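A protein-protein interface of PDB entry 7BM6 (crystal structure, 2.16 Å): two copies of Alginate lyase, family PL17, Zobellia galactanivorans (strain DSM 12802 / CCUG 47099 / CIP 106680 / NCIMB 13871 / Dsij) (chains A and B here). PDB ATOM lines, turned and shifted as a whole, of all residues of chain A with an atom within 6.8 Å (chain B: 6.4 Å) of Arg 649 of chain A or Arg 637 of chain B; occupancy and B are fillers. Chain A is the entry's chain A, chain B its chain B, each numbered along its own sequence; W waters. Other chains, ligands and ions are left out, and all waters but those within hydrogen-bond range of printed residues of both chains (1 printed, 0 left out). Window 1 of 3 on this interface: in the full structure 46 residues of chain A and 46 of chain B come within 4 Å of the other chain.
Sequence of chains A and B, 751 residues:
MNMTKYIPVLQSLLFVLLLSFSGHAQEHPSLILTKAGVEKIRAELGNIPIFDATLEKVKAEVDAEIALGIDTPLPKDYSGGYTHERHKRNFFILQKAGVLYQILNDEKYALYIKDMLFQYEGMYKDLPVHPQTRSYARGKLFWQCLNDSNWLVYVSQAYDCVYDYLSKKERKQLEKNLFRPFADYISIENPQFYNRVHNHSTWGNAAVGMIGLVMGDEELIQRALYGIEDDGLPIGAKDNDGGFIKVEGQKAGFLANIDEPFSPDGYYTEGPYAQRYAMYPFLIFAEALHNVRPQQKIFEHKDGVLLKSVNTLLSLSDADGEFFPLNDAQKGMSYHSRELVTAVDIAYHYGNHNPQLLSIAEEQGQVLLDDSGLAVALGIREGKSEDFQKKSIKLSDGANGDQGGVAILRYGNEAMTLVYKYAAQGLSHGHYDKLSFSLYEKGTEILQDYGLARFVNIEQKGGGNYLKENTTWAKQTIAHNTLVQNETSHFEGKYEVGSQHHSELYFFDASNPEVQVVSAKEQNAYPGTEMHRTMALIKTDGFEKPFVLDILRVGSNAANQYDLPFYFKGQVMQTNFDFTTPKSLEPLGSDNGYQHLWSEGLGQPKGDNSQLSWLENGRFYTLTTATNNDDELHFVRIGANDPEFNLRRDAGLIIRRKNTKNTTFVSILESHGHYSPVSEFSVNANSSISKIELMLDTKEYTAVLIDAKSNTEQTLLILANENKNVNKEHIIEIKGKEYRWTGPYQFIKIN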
ATOM      1  N   TYR A 450     -31.470  33.043 -18.586  1.00  0.00           N
ATOM      2  CA  TYR A 450     -31.686  31.744 -17.980  1.00  0.00           C
ATOM      3  C   TYR A 450     -32.023  30.648 -18.971  1.00  0.00           C
ATOM      4  O   TYR A 450     -31.672  29.473 -18.728  1.00  0.00           O
ATOM      5  CB  TYR A 450     -32.733  31.784 -16.861  1.00  0.00           C
ATOM      6  CG  TYR A 450     -32.807  30.523 -16.064  1.00  0.00           C
ATOM      7  CD1 TYR A 450     -33.612  29.486 -16.476  1.00  0.00           C
ATOM      8  CD2 TYR A 450     -32.019  30.334 -14.938  1.00  0.00           C
ATOM      9  CE1 TYR A 450     -33.656  28.269 -15.794  1.00  0.00           C
ATOM     10  CE2 TYR A 450     -32.054  29.134 -14.207  1.00  0.00           C
ATOM     11  CZ  TYR A 450     -32.854  28.091 -14.656  1.00  0.00           C
ATOM     12  OH  TYR A 450     -32.937  26.866 -14.012  1.00  0.00           O
ATOM     13  N   TRP A 598     -33.729  32.841  -3.186  1.00  0.00           N
ATOM     14  CA  TRP A 598     -33.328  32.928  -1.784  1.00  0.00           C
ATOM     15  C   TRP A 598     -32.513  34.224  -1.606  1.00  0.00           C
ATOM     16  O   TRP A 598     -31.630  34.519  -2.423  1.00  0.00           O
ATOM     17  CB  TRP A 598     -32.421  31.757  -1.413  1.00  0.00           C
ATOM     18  CG  TRP A 598     -32.982  30.378  -1.455  1.00  0.00           C
ATOM     19  CD1 TRP A 598     -32.535  29.287  -2.223  1.00  0.00           C
ATOM     20  CD2 TRP A 598     -34.059  29.904  -0.667  1.00  0.00           C
ATOM     21  NE1 TRP A 598     -33.282  28.164  -1.886  1.00  0.00           N
ATOM     22  CE2 TRP A 598     -34.235  28.528  -0.965  1.00  0.00           C
ATOM     23  CE3 TRP A 598     -34.887  30.508   0.244  1.00  0.00           C
ATOM     24  CZ2 TRP A 598     -35.221  27.779  -0.396  1.00  0.00           C
ATOM     25  CZ3 TRP A 598     -35.849  29.749   0.849  1.00  0.00           C
ATOM     26  CH2 TRP A 598     -36.037  28.419   0.516  1.00  0.00           C
ATOM     27  N   ARG A 637     -29.940  33.670  -4.769  1.00  0.00           N
ATOM     28  CA  ARG A 637     -29.679  32.338  -5.306  1.00  0.00           C
ATOM     29  C   ARG A 637     -30.993  31.686  -5.770  1.00  0.00           C
ATOM     30  O   ARG A 637     -31.983  31.656  -5.035  1.00  0.00           O
ATOM     31  CB  ARG A 637     -28.994  31.573  -4.185  1.00  0.00           C
ATOM     32  CG  ARG A 637     -28.893  30.070  -4.284  1.00  0.00           C
ATOM     33  CD  ARG A 637     -27.560  29.574  -4.752  1.00  0.00           C
ATOM     34  NE  ARG A 637     -26.409  30.265  -4.171  1.00  0.00           N
ATOM     35  CZ  ARG A 637     -25.240  30.412  -4.797  1.00  0.00           C
ATOM     36  NH1 ARG A 637     -25.056  29.852  -6.006  1.00  0.00           N
ATOM     37  NH2 ARG A 637     -24.252  31.098  -4.208  1.00  0.00           N
ATOM     38  N   ILE A 638     -31.007  31.193  -6.998  1.00  0.00           N
ATOM     39  CA  ILE A 638     -32.190  30.612  -7.572  1.00  0.00           C
ATOM     40  C   ILE A 638     -32.388  29.258  -6.877  1.00  0.00           C
ATOM     41  O   ILE A 638     -31.400  28.560  -6.600  1.00  0.00           O
ATOM     42  CB  ILE A 638     -32.038  30.445  -9.083  1.00  0.00           C
ATOM     43  CG1 ILE A 638     -31.874  31.775  -9.782  1.00  0.00           C
ATOM     44  CG2 ILE A 638     -33.232  29.713  -9.669  1.00  0.00           C
ATOM     45  CD1 ILE A 638     -31.242  31.624 -11.166  1.00  0.00           C
ATOM     46  N   GLY A 639     -33.638  28.918  -6.546  1.00  0.00           N
ATOM     47  CA  GLY A 639     -33.955  27.608  -5.990  1.00  0.00           C
ATOM     48  C   GLY A 639     -35.039  27.503  -4.946  1.00  0.00           C
ATOM     49  O   GLY A 639     -35.380  26.367  -4.562  1.00  0.00           O
ATOM     50  N   ALA A 640     -35.584  28.634  -4.465  1.00  0.00           N
ATOM     51  CA  ALA A 640     -36.742  28.604  -3.597  1.00  0.00           C
ATOM     52  C   ALA A 640     -37.989  28.084  -4.340  1.00  0.00           C
ATOM     53  O   ALA A 640     -38.101  28.231  -5.568  1.00  0.00           O
ATOM     54  CB  ALA A 640     -37.012  29.974  -2.985  1.00  0.00           C
ATOM     55  N   ASN A 641     -38.948  27.543  -3.573  1.00  0.00           N
ATOM     56  CA  ASN A 641     -40.203  27.033  -4.083  1.00  0.00           C
ATOM     57  C   ASN A 641     -39.957  26.187  -5.385  1.00  0.00           C
ATOM     58  O   ASN A 641     -40.539  26.453  -6.452  1.00  0.00           O
ATOM     59  CB  ASN A 641     -41.193  28.191  -4.317  1.00  0.00           C
ATOM     60  CG  ASN A 641     -41.741  28.779  -3.006  1.00  0.00           C
ATOM     61  OD1 ASN A 641     -42.464  28.092  -2.265  1.00  0.00           O
ATOM     62  ND2 ASN A 641     -41.393  30.031  -2.706  1.00  0.00           N
ATOM     63  N   ASP A 642     -39.054  25.214  -5.262  1.00  0.00           N
ATOM     64  CA  ASP A 642     -38.642  24.320  -6.371  1.00  0.00           C
ATOM     65  C   ASP A 642     -38.679  22.871  -5.889  1.00  0.00           C
ATOM     66  O   ASP A 642     -37.656  22.208  -5.784  1.00  0.00           O
ATOM     67  CB  ASP A 642     -37.235  24.691  -6.882  1.00  0.00           C
ATOM     68  CG  ASP A 642     -36.806  23.867  -8.094  1.00  0.00           C
ATOM     69  OD1 ASP A 642     -37.670  23.308  -8.850  1.00  0.00           O
ATOM     70  OD2 ASP A 642     -35.596  23.737  -8.303  1.00  0.00           O
ATOM     71  N   PRO A 643     -39.870  22.362  -5.585  1.00  0.00           N
ATOM     72  CA  PRO A 643     -39.977  21.047  -4.913  1.00  0.00           C
ATOM     73  C   PRO A 643     -39.374  19.839  -5.676  1.00  0.00           C
ATOM     74  O   PRO A 643     -39.116  18.831  -5.057  1.00  0.00           O
ATOM     75  CB  PRO A 643     -41.512  20.858  -4.719  1.00  0.00           C
ATOM     76  CG  PRO A 643     -42.149  21.819  -5.686  1.00  0.00           C
ATOM     77  CD  PRO A 643     -41.186  22.983  -5.817  1.00  0.00           C
ATOM     78  N   GLU A 644     -39.126  19.953  -6.976  1.00  0.00           N
ATOM     79  CA  GLU A 644     -38.632  18.823  -7.792  1.00  0.00           C
ATOM     80  C   GLU A 644     -37.233  19.029  -8.373  1.00  0.00           C
ATOM     81  O   GLU A 644     -36.811  18.272  -9.265  1.00  0.00           O
ATOM     82  CB  GLU A 644     -39.616  18.563  -8.941  1.00  0.00           C
ATOM     83  CG  GLU A 644     -41.052  18.394  -8.470  1.00  0.00           C
ATOM     84  CD  GLU A 644     -42.021  18.122  -9.611  1.00  0.00           C
ATOM     85  OE1 GLU A 644     -42.100  18.900 -10.611  1.00  0.00           O
ATOM     86  OE2 GLU A 644     -42.717  17.102  -9.502  1.00  0.00           O
ATOM     87  N   PHE A 645     -36.532  20.035  -7.852  1.00  0.00           N
ATOM     88  CA  PHE A 645     -35.215  20.416  -8.270  1.00  0.00           C
ATOM     89  C   PHE A 645     -35.244  20.649  -9.801  1.00  0.00           C
ATOM     90  O   PHE A 645     -34.477  20.047 -10.576  1.00  0.00           O
ATOM     91  CB  PHE A 645     -34.173  19.371  -7.864  1.00  0.00           C
ATOM     92  CG  PHE A 645     -33.885  19.305  -6.396  1.00  0.00           C
ATOM     93  CD1 PHE A 645     -33.112  20.295  -5.768  1.00  0.00           C
ATOM     94  CD2 PHE A 645     -34.331  18.217  -5.628  1.00  0.00           C
ATOM     95  CE1 PHE A 645     -32.847  20.213  -4.386  1.00  0.00           C
ATOM     96  CE2 PHE A 645     -34.080  18.154  -4.261  1.00  0.00           C
ATOM     97  CZ  PHE A 645     -33.329  19.131  -3.652  1.00  0.00           C
ATOM     98  N   ASN A 646     -36.166  21.472 -10.242  1.00  0.00           N
ATOM     99  CA  ASN A 646     -36.289  21.803 -11.652  1.00  0.00           C
ATOM    100  C   ASN A 646     -35.447  22.998 -12.048  1.00  0.00           C
ATOM    101  O   ASN A 646     -35.297  23.245 -13.267  1.00  0.00           O
ATOM    102  CB  ASN A 646     -37.742  22.057 -12.052  1.00  0.00           C
ATOM    103  CG  ASN A 646     -38.599  20.803 -12.064  1.00  0.00           C
ATOM    104  OD1 ASN A 646     -38.134  19.682 -12.295  1.00  0.00           O
ATOM    105  ND2 ASN A 646     -39.881  20.998 -11.860  1.00  0.00           N
ATOM    106  N   LEU A 647     -34.887  23.706 -11.065  1.00  0.00           N
ATOM    107  CA  LEU A 647     -34.132  24.947 -11.307  1.00  0.00           C
ATOM    108  C   LEU A 647     -32.678  24.797 -10.843  1.00  0.00           C
ATOM    109  O   LEU A 647     -32.358  24.052  -9.863  1.00  0.00           O
ATOM    110  CB  LEU A 647     -34.771  26.138 -10.565  1.00  0.00           C
ATOM    111  CG  LEU A 647     -36.196  26.525 -11.007  1.00  0.00           C
ATOM    112  CD1 LEU A 647     -36.730  27.635 -10.131  1.00  0.00           C
ATOM    113  CD2 LEU A 647     -36.346  26.933 -12.470  1.00  0.00           C
ATOM    114  N   ARG A 648     -31.808  25.509 -11.546  1.00  0.00           N
ATOM    115  CA  ARG A 648     -30.415  25.557 -11.236  1.00  0.00           C
ATOM    116  C   ARG A 648     -30.155  26.506 -10.050  1.00  0.00           C
ATOM    117  O   ARG A 648     -30.765  27.558  -9.949  1.00  0.00           O
ATOM    118  CB  ARG A 648     -29.640  26.022 -12.465  1.00  0.00           C
ATOM    119  CG  ARG A 648     -29.632  25.055 -13.639  1.00  0.00           C
ATOM    120  CD  ARG A 648     -28.577  25.473 -14.667  1.00  0.00           C
ATOM    121  NE  ARG A 648     -28.786  26.830 -15.195  1.00  0.00           N
ATOM    122  CZ  ARG A 648     -29.616  27.181 -16.193  1.00  0.00           C
ATOM    123  NH1 ARG A 648     -30.468  26.289 -16.757  1.00  0.00           N
ATOM    124  NH2 ARG A 648     -29.649  28.463 -16.609  1.00  0.00           N
ATOM    125  N   ARG A 649     -29.192  26.172  -9.202  1.00  0.00           N
ATOM    126  CA  ARG A 649     -28.798  27.044  -8.105  1.00  0.00           C
ATOM    127  C   ARG A 649     -27.760  28.114  -8.466  1.00  0.00           C
ATOM    128  O   ARG A 649     -26.783  28.265  -7.767  1.00  0.00           O
ATOM    129  CB  ARG A 649     -28.355  26.215  -6.949  1.00  0.00           C
ATOM    130  CG  ARG A 649     -29.458  25.890  -5.978  1.00  0.00           C
ATOM    131  CD  ARG A 649     -30.517  25.031  -6.568  1.00  0.00           C
ATOM    132  NE  ARG A 649     -31.532  24.634  -5.572  1.00  0.00           N
ATOM    133  CZ  ARG A 649     -32.725  24.151  -5.899  1.00  0.00           C
ATOM    134  NH1 ARG A 649     -33.120  24.079  -7.180  1.00  0.00           N
ATOM    135  NH2 ARG A 649     -33.565  23.779  -4.953  1.00  0.00           N
ATOM    136  N   ASP A 650     -28.031  28.883  -9.527  1.00  0.00           N
ATOM    137  CA  ASP A 650     -27.172  29.963  -9.991  1.00  0.00           C
ATOM    138  C   ASP A 650     -27.419  31.170  -9.081  1.00  0.00           C
ATOM    139  O   ASP A 650     -28.504  31.300  -8.494  1.00  0.00           O
ATOM    140  CB  ASP A 650     -27.513  30.331 -11.436  1.00  0.00           C
ATOM    141  CG  ASP A 650     -27.218  29.184 -12.446  1.00  0.00           C
ATOM    142  OD1 ASP A 650     -26.302  28.396 -12.219  1.00  0.00           O
ATOM    143  OD2 ASP A 650     -27.898  29.067 -13.494  1.00  0.00           O
ATOM    144  N   ALA A 651     -26.412  32.041  -8.978  1.00  0.00           N
ATOM    145  CA  ALA A 651     -26.495  33.259  -8.166  1.00  0.00           C
ATOM    146  C   ALA A 651     -26.783  34.512  -8.972  1.00  0.00           C
ATOM    147  O   ALA A 651     -26.684  34.515 -10.201  1.00  0.00           O
ATOM    148  CB  ALA A 651     -25.191  33.443  -7.450  1.00  0.00           C
ATOM    149  N   LEU B 585     -34.645  27.872   4.326  1.00  0.00           N
ATOM    150  CA  LEU B 585     -33.505  26.995   4.621  1.00  0.00           C
ATOM    151  C   LEU B 585     -32.828  27.315   5.990  1.00  0.00           C
ATOM    152  O   LEU B 585     -32.382  28.443   6.251  1.00  0.00           O
ATOM    153  CB  LEU B 585     -32.457  27.013   3.495  1.00  0.00           C
ATOM    154  CG  LEU B 585     -32.894  26.727   2.040  1.00  0.00           C
ATOM    155  CD1 LEU B 585     -31.680  26.548   1.176  1.00  0.00           C
ATOM    156  CD2 LEU B 585     -33.760  25.507   1.877  1.00  0.00           C
ATOM    157  N   HIS B 596     -22.394  24.329   8.295  1.00  0.00           N
ATOM    158  CA  HIS B 596     -22.184  24.771   6.932  1.00  0.00           C
ATOM    159  C   HIS B 596     -23.138  24.134   5.897  1.00  0.00           C
ATOM    160  O   HIS B 596     -23.045  24.464   4.716  1.00  0.00           O
ATOM    161  CB  HIS B 596     -20.719  24.514   6.526  1.00  0.00           C
ATOM    162  CG  HIS B 596     -19.738  25.345   7.301  1.00  0.00           C
ATOM    163  ND1 HIS B 596     -19.783  26.726   7.309  1.00  0.00           N
ATOM    164  CD2 HIS B 596     -18.673  25.000   8.052  1.00  0.00           C
ATOM    165  CE1 HIS B 596     -18.783  27.193   8.035  1.00  0.00           C
ATOM    166  NE2 HIS B 596     -18.102  26.167   8.505  1.00  0.00           N
ATOM    167  N   LEU B 597     -24.064  23.268   6.345  1.00  0.00           N
ATOM    168  CA  LEU B 597     -25.056  22.667   5.436  1.00  0.00           C
ATOM    169  C   LEU B 597     -26.462  23.208   5.586  1.00  0.00           C
ATOM    170  O   LEU B 597     -27.052  23.126   6.677  1.00  0.00           O
ATOM    171  CB  LEU B 597     -25.103  21.162   5.651  1.00  0.00           C
ATOM    172  CG  LEU B 597     -23.860  20.361   5.325  1.00  0.00           C
ATOM    173  CD1 LEU B 597     -23.984  18.933   5.831  1.00  0.00           C
ATOM    174  CD2 LEU B 597     -23.624  20.384   3.807  1.00  0.00           C
ATOM    175  N   TRP B 598     -27.023  23.740   4.488  1.00  0.00           N
ATOM    176  CA  TRP B 598     -28.453  24.037   4.457  1.00  0.00           C
ATOM    177  C   TRP B 598     -29.272  22.725   4.274  1.00  0.00           C
ATOM    178  O   TRP B 598     -28.926  21.838   3.451  1.00  0.00           O
ATOM    179  CB  TRP B 598     -28.812  25.005   3.354  1.00  0.00           C
ATOM    180  CG  TRP B 598     -28.159  26.398   3.342  1.00  0.00           C
ATOM    181  CD1 TRP B 598     -27.337  26.913   2.368  1.00  0.00           C
ATOM    182  CD2 TRP B 598     -28.354  27.413   4.290  1.00  0.00           C
ATOM    183  NE1 TRP B 598     -27.013  28.214   2.669  1.00  0.00           N
ATOM    184  CE2 TRP B 598     -27.611  28.539   3.865  1.00  0.00           C
ATOM    185  CE3 TRP B 598     -29.089  27.493   5.461  1.00  0.00           C
ATOM    186  CZ2 TRP B 598     -27.576  29.703   4.569  1.00  0.00           C
ATOM    187  CZ3 TRP B 598     -29.050  28.691   6.188  1.00  0.00           C
ATOM    188  CH2 TRP B 598     -28.300  29.767   5.739  1.00  0.00           C
ATOM    189  N   SER B 599     -30.336  22.617   5.059  1.00  0.00           N
ATOM    190  CA  SER B 599     -31.298  21.537   4.947  1.00  0.00           C
ATOM    191  C   SER B 599     -32.288  21.857   3.803  1.00  0.00           C
ATOM    192  O   SER B 599     -33.198  22.708   3.948  1.00  0.00           O
ATOM    193  CB  SER B 599     -32.021  21.372   6.290  1.00  0.00           C
ATOM    194  OG  SER B 599     -32.842  20.248   6.268  1.00  0.00           O
ATOM    195  N   GLU B 600     -32.119  21.184   2.679  1.00  0.00           N
ATOM    196  CA  GLU B 600     -32.844  21.537   1.476  1.00  0.00           C
ATOM    197  C   GLU B 600     -34.052  20.638   1.206  1.00  0.00           C
ATOM    198  O   GLU B 600     -34.848  20.939   0.348  1.00  0.00           O
ATOM    199  CB  GLU B 600     -31.859  21.512   0.283  1.00  0.00           C
ATOM    200  CG  GLU B 600     -32.210  22.450  -0.823  1.00  0.00           C
ATOM    201  CD  GLU B 600     -31.082  22.688  -1.866  1.00  0.00           C
ATOM    202  OE1 GLU B 600     -30.306  21.771  -2.262  1.00  0.00           O
ATOM    203  OE2 GLU B 600     -31.002  23.850  -2.305  1.00  0.00           O
ATOM    204  N   PHE B 635     -31.675  15.876   1.700  1.00  0.00           N
ATOM    205  CA  PHE B 635     -31.032  16.709   0.709  1.00  0.00           C
ATOM    206  C   PHE B 635     -30.383  17.905   1.427  1.00  0.00           C
ATOM    207  O   PHE B 635     -31.055  18.572   2.238  1.00  0.00           O
ATOM    208  CB  PHE B 635     -32.038  17.223  -0.319  1.00  0.00           C
ATOM    209  CG  PHE B 635     -32.428  16.217  -1.334  1.00  0.00           C
ATOM    210  CD1 PHE B 635     -31.535  15.858  -2.365  1.00  0.00           C
ATOM    211  CD2 PHE B 635     -33.680  15.609  -1.284  1.00  0.00           C
ATOM    212  CE1 PHE B 635     -31.914  14.910  -3.317  1.00  0.00           C
ATOM    213  CE2 PHE B 635     -34.044  14.670  -2.238  1.00  0.00           C
ATOM    214  CZ  PHE B 635     -33.165  14.325  -3.256  1.00  0.00           C
ATOM    215  N   VAL B 636     -29.102  18.134   1.126  1.00  0.00           N
ATOM    216  CA  VAL B 636     -28.292  19.214   1.713  1.00  0.00           C
ATOM    217  C   VAL B 636     -27.613  20.057   0.653  1.00  0.00           C
ATOM    218  O   VAL B 636     -27.426  19.584  -0.464  1.00  0.00           O
ATOM    219  CB  VAL B 636     -27.226  18.760   2.745  1.00  0.00           C
ATOM    220  CG1 VAL B 636     -27.914  18.127   3.971  1.00  0.00           C
ATOM    221  CG2 VAL B 636     -26.167  17.825   2.188  1.00  0.00           C
ATOM    222  N   ARG B 637     -27.299  21.310   1.017  1.00  0.00           N
ATOM    223  CA  ARG B 637     -26.521  22.212   0.201  1.00  0.00           C
ATOM    224  C   ARG B 637     -25.468  22.951   1.055  1.00  0.00           C
ATOM    225  O   ARG B 637     -25.778  23.571   2.118  1.00  0.00           O
ATOM    226  CB  ARG B 637     -27.394  23.250  -0.539  1.00  0.00           C
ATOM    227  CG  ARG B 637     -26.597  23.811  -1.731  1.00  0.00           C
ATOM    228  CD  ARG B 637     -27.389  24.479  -2.770  1.00  0.00           C
ATOM    229  NE  ARG B 637     -28.292  23.547  -3.410  1.00  0.00           N
ATOM    230  CZ  ARG B 637     -28.020  22.784  -4.456  1.00  0.00           C
ATOM    231  NH1 ARG B 637     -26.824  22.828  -5.104  1.00  0.00           N
ATOM    232  NH2 ARG B 637     -29.016  22.018  -4.907  1.00  0.00           N
ATOM    233  N   ILE B 638     -24.242  22.899   0.586  1.00  0.00           N
ATOM    234  CA  ILE B 638     -23.137  23.574   1.258  1.00  0.00           C
ATOM    235  C   ILE B 638     -23.326  25.079   1.054  1.00  0.00           C
ATOM    236  O   ILE B 638     -23.775  25.521  -0.014  1.00  0.00           O
ATOM    237  CB  ILE B 638     -21.769  23.094   0.692  1.00  0.00           C
ATOM    238  CG1 ILE B 638     -21.602  21.592   0.875  1.00  0.00           C
ATOM    239  CG2 ILE B 638     -20.583  23.799   1.354  1.00  0.00           C
ATOM    240  CD1 ILE B 638     -20.544  21.054  -0.059  1.00  0.00           C
ATOM    241  N   GLY B 639     -23.017  25.865   2.074  1.00  0.00           N
ATOM    242  CA  GLY B 639     -23.051  27.350   1.928  1.00  0.00           C
ATOM    243  C   GLY B 639     -23.574  28.116   3.114  1.00  0.00           C
ATOM    244  O   GLY B 639     -23.441  29.313   3.117  1.00  0.00           O
ATOM    245  N   ALA B 640     -24.118  27.444   4.128  1.00  0.00           N
ATOM    246  CA  ALA B 640     -24.472  28.095   5.390  1.00  0.00           C
ATOM    247  C   ALA B 640     -23.232  28.565   6.195  1.00  0.00           C
ATOM    248  O   ALA B 640     -22.157  27.952   6.113  1.00  0.00           O
ATOM    249  CB  ALA B 640     -25.340  27.190   6.232  1.00  0.00           C
ATOM    250  N   ARG B 648     -18.152  26.305  -2.038  1.00  0.00           N
ATOM    251  CA  ARG B 648     -18.959  26.019  -3.197  1.00  0.00           C
ATOM    252  C   ARG B 648     -20.396  25.564  -2.789  1.00  0.00           C
ATOM    253  O   ARG B 648     -20.548  24.817  -1.845  1.00  0.00           O
ATOM    254  CB  ARG B 648     -18.320  24.922  -4.049  1.00  0.00           C
ATOM    255  CG  ARG B 648     -17.009  25.335  -4.700  1.00  0.00           C
ATOM    256  CD  ARG B 648     -16.538  24.259  -5.661  1.00  0.00           C
ATOM    257  NE  ARG B 648     -16.360  22.950  -5.021  1.00  0.00           N
ATOM    258  CZ  ARG B 648     -15.304  22.515  -4.325  1.00  0.00           C
ATOM    259  NH1 ARG B 648     -14.252  23.294  -4.072  1.00  0.00           N
ATOM    260  NH2 ARG B 648     -15.288  21.248  -3.850  1.00  0.00           N
ATOM    261  N   ARG B 649     -21.407  25.921  -3.587  1.00  0.00           N
ATOM    262  CA  ARG B 649     -22.781  25.514  -3.347  1.00  0.00           C
ATOM    263  C   ARG B 649     -23.135  24.132  -3.936  1.00  0.00           C
ATOM    264  O   ARG B 649     -24.136  23.995  -4.598  1.00  0.00           O
ATOM    265  CB  ARG B 649     -23.758  26.595  -3.806  1.00  0.00           C
ATOM    266  CG  ARG B 649     -24.128  27.574  -2.723  1.00  0.00           C
ATOM    267  CD  ARG B 649     -22.991  28.444  -2.286  1.00  0.00           C
ATOM    268  NE  ARG B 649     -23.420  29.467  -1.290  1.00  0.00           N
ATOM    269  CZ  ARG B 649     -22.599  30.031  -0.389  1.00  0.00           C
ATOM    270  NH1 ARG B 649     -21.337  29.624  -0.244  1.00  0.00           N
ATOM    271  NH2 ARG B 649     -23.043  30.979   0.431  1.00  0.00           N
ATOM    272  N   ASP B 650     -22.305  23.128  -3.638  1.00  0.00           N
ATOM    273  CA  ASP B 650     -22.501  21.759  -4.054  1.00  0.00           C
ATOM    274  C   ASP B 650     -23.563  21.096  -3.139  1.00  0.00           C
ATOM    275  O   ASP B 650     -23.783  21.505  -1.997  1.00  0.00           O
ATOM    276  CB  ASP B 650     -21.195  20.967  -3.945  1.00  0.00           C
ATOM    277  CG  ASP B 650     -20.068  21.499  -4.862  1.00  0.00           C
ATOM    278  OD1 ASP B 650     -20.337  22.021  -5.952  1.00  0.00           O
ATOM    279  OD2 ASP B 650     -18.879  21.377  -4.487  1.00  0.00           O
ATOM    280  N   ALA B 651     -24.198  20.055  -3.651  1.00  0.00           N
ATOM    281  CA  ALA B 651     -25.279  19.357  -2.925  1.00  0.00           C
ATOM    282  C   ALA B 651     -24.876  17.983  -2.408  1.00  0.00           C
ATOM    283  O   ALA B 651     -23.814  17.443  -2.723  1.00  0.00           O
ATOM    284  CB  ALA B 651     -26.477  19.244  -3.805  1.00  0.00           C
ATOM    285  N   GLY B 652     -25.717  17.415  -1.593  1.00  0.00           N
ATOM    286  CA  GLY B 652     -25.521  16.038  -1.172  1.00  0.00           C
ATOM    287  C   GLY B 652     -26.820  15.452  -0.711  1.00  0.00           C
ATOM    288  O   GLY B 652     -27.791  16.170  -0.542  1.00  0.00           O
HETATM  289  O   HOH W   1     -33.141  25.543  -2.178  1.00  0.00           O
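The guanidinium group (NE) of Arg 649 of chain A lies within salt-bridge range of the side-chain carboxylate (OE2) of Glu 600 of chain B (3.4 Å). NH2 of Arg 637 of chain A sits close to NE of Arg 649 of chain B (3.4 Å).
The side-chain carboxylate of Asp 642 of chain A is in salt-bridge range of the guanidinium group of Arg 649 of chain A, at 2.7 Å. The backbone NH (N) of Trp 598 of chain B is in hydrogen-bond range of the backbone carbonyl oxygen (O) of Arg 637 of chain B, at 2.7 Å. O of Leu 647 of chain A sits at hydrogen-bond distance from NH1 of Arg 649 of chain A. O of Gly 639 of chain A lies within hydrogen-bond range of NH2 of Arg 649 of chain A. The backbone carbonyl oxygen (O) of Arg 637 of chain A sits at hydrogen-bond distance from the backbone NH (N) of Trp 598 of chain A (2.8 Å). The backbone carbonyl oxygen (O) of Phe 635 of chain B is in hydrogen-bond range of the backbone NH (N) of Glu 600 of chain B.
Leu 585 of chain B touches Trp 598 of chain A (CG to CZ2, 3.5 Å). OE1 of Glu 600 of chain B touches CE1 of Phe 645 of chain A, 3.7 Å away. Phe 635 of chain B touches Phe 645 of chain A. Arg 649 of chain A touches Arg 637 of chain B (CG to NE, 3.7 Å).
Of the printed residues of chain B, Trp 598 of chain A touches Leu 585. Of the printed residues of chain B, Phe 645 of chain A touches Glu 600 and Phe 635. Arg 649 of chain A touches two residues of chain B. Printed residues of chain A within 4 Å of Leu 585 of chain B: Trp 598 (3.5 Å). Of the printed residues of chain A, Glu 600 of chain B touches Phe 645 (3.7 Å) and Arg 649 (3.4 Å). Of chain A, only Arg 649 comes within 4 Å of Arg 637 of chain B. The nearest residue of chain A that does not touch Arg 637 of chain B is Phe 645 of chain A (4.3 Å). The nearest printed residue of chain B that does not touch Trp 598 of chain A is Glu 600 of chain B (4.9 Å).
Printed residues of chain A that touch a printed residue of chain B: Trp 598, Arg 637, Phe 645 and Arg 649. Hydrophobic or aromatic side chains of chain A that line the printed part of chain B: Trp 598 and Phe 645. Along chain A the printed residues that touch a printed residue of chain B span positions 598 to 649. Of the 17 printed residues of chain B, 5 touch a printed residue of chain A. Hydrophobic or aromatic side chains of chain B that line the printed part of chain A: Leu 585 and Phe 635.
Arg 637 of chain A touches Arg 649 of chain B, and with the chains exchanged Arg 649 of chain A touches Arg 637 of chain B. 9 positions are printed for both chains. Of the 6 pairs that touch across the chains among the printed residues, 2 have their exchanged pair printed and touching as well.
Water W1 lies within hydrogen-bond range of the indole nitrogen of Trp 598 of chain A, the side-chain carboxylate of Glu 600 of chain B, the guanidinium group of Arg 649 of chain A and the backbone carbonyl oxygen of Gly 639 of chain A.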
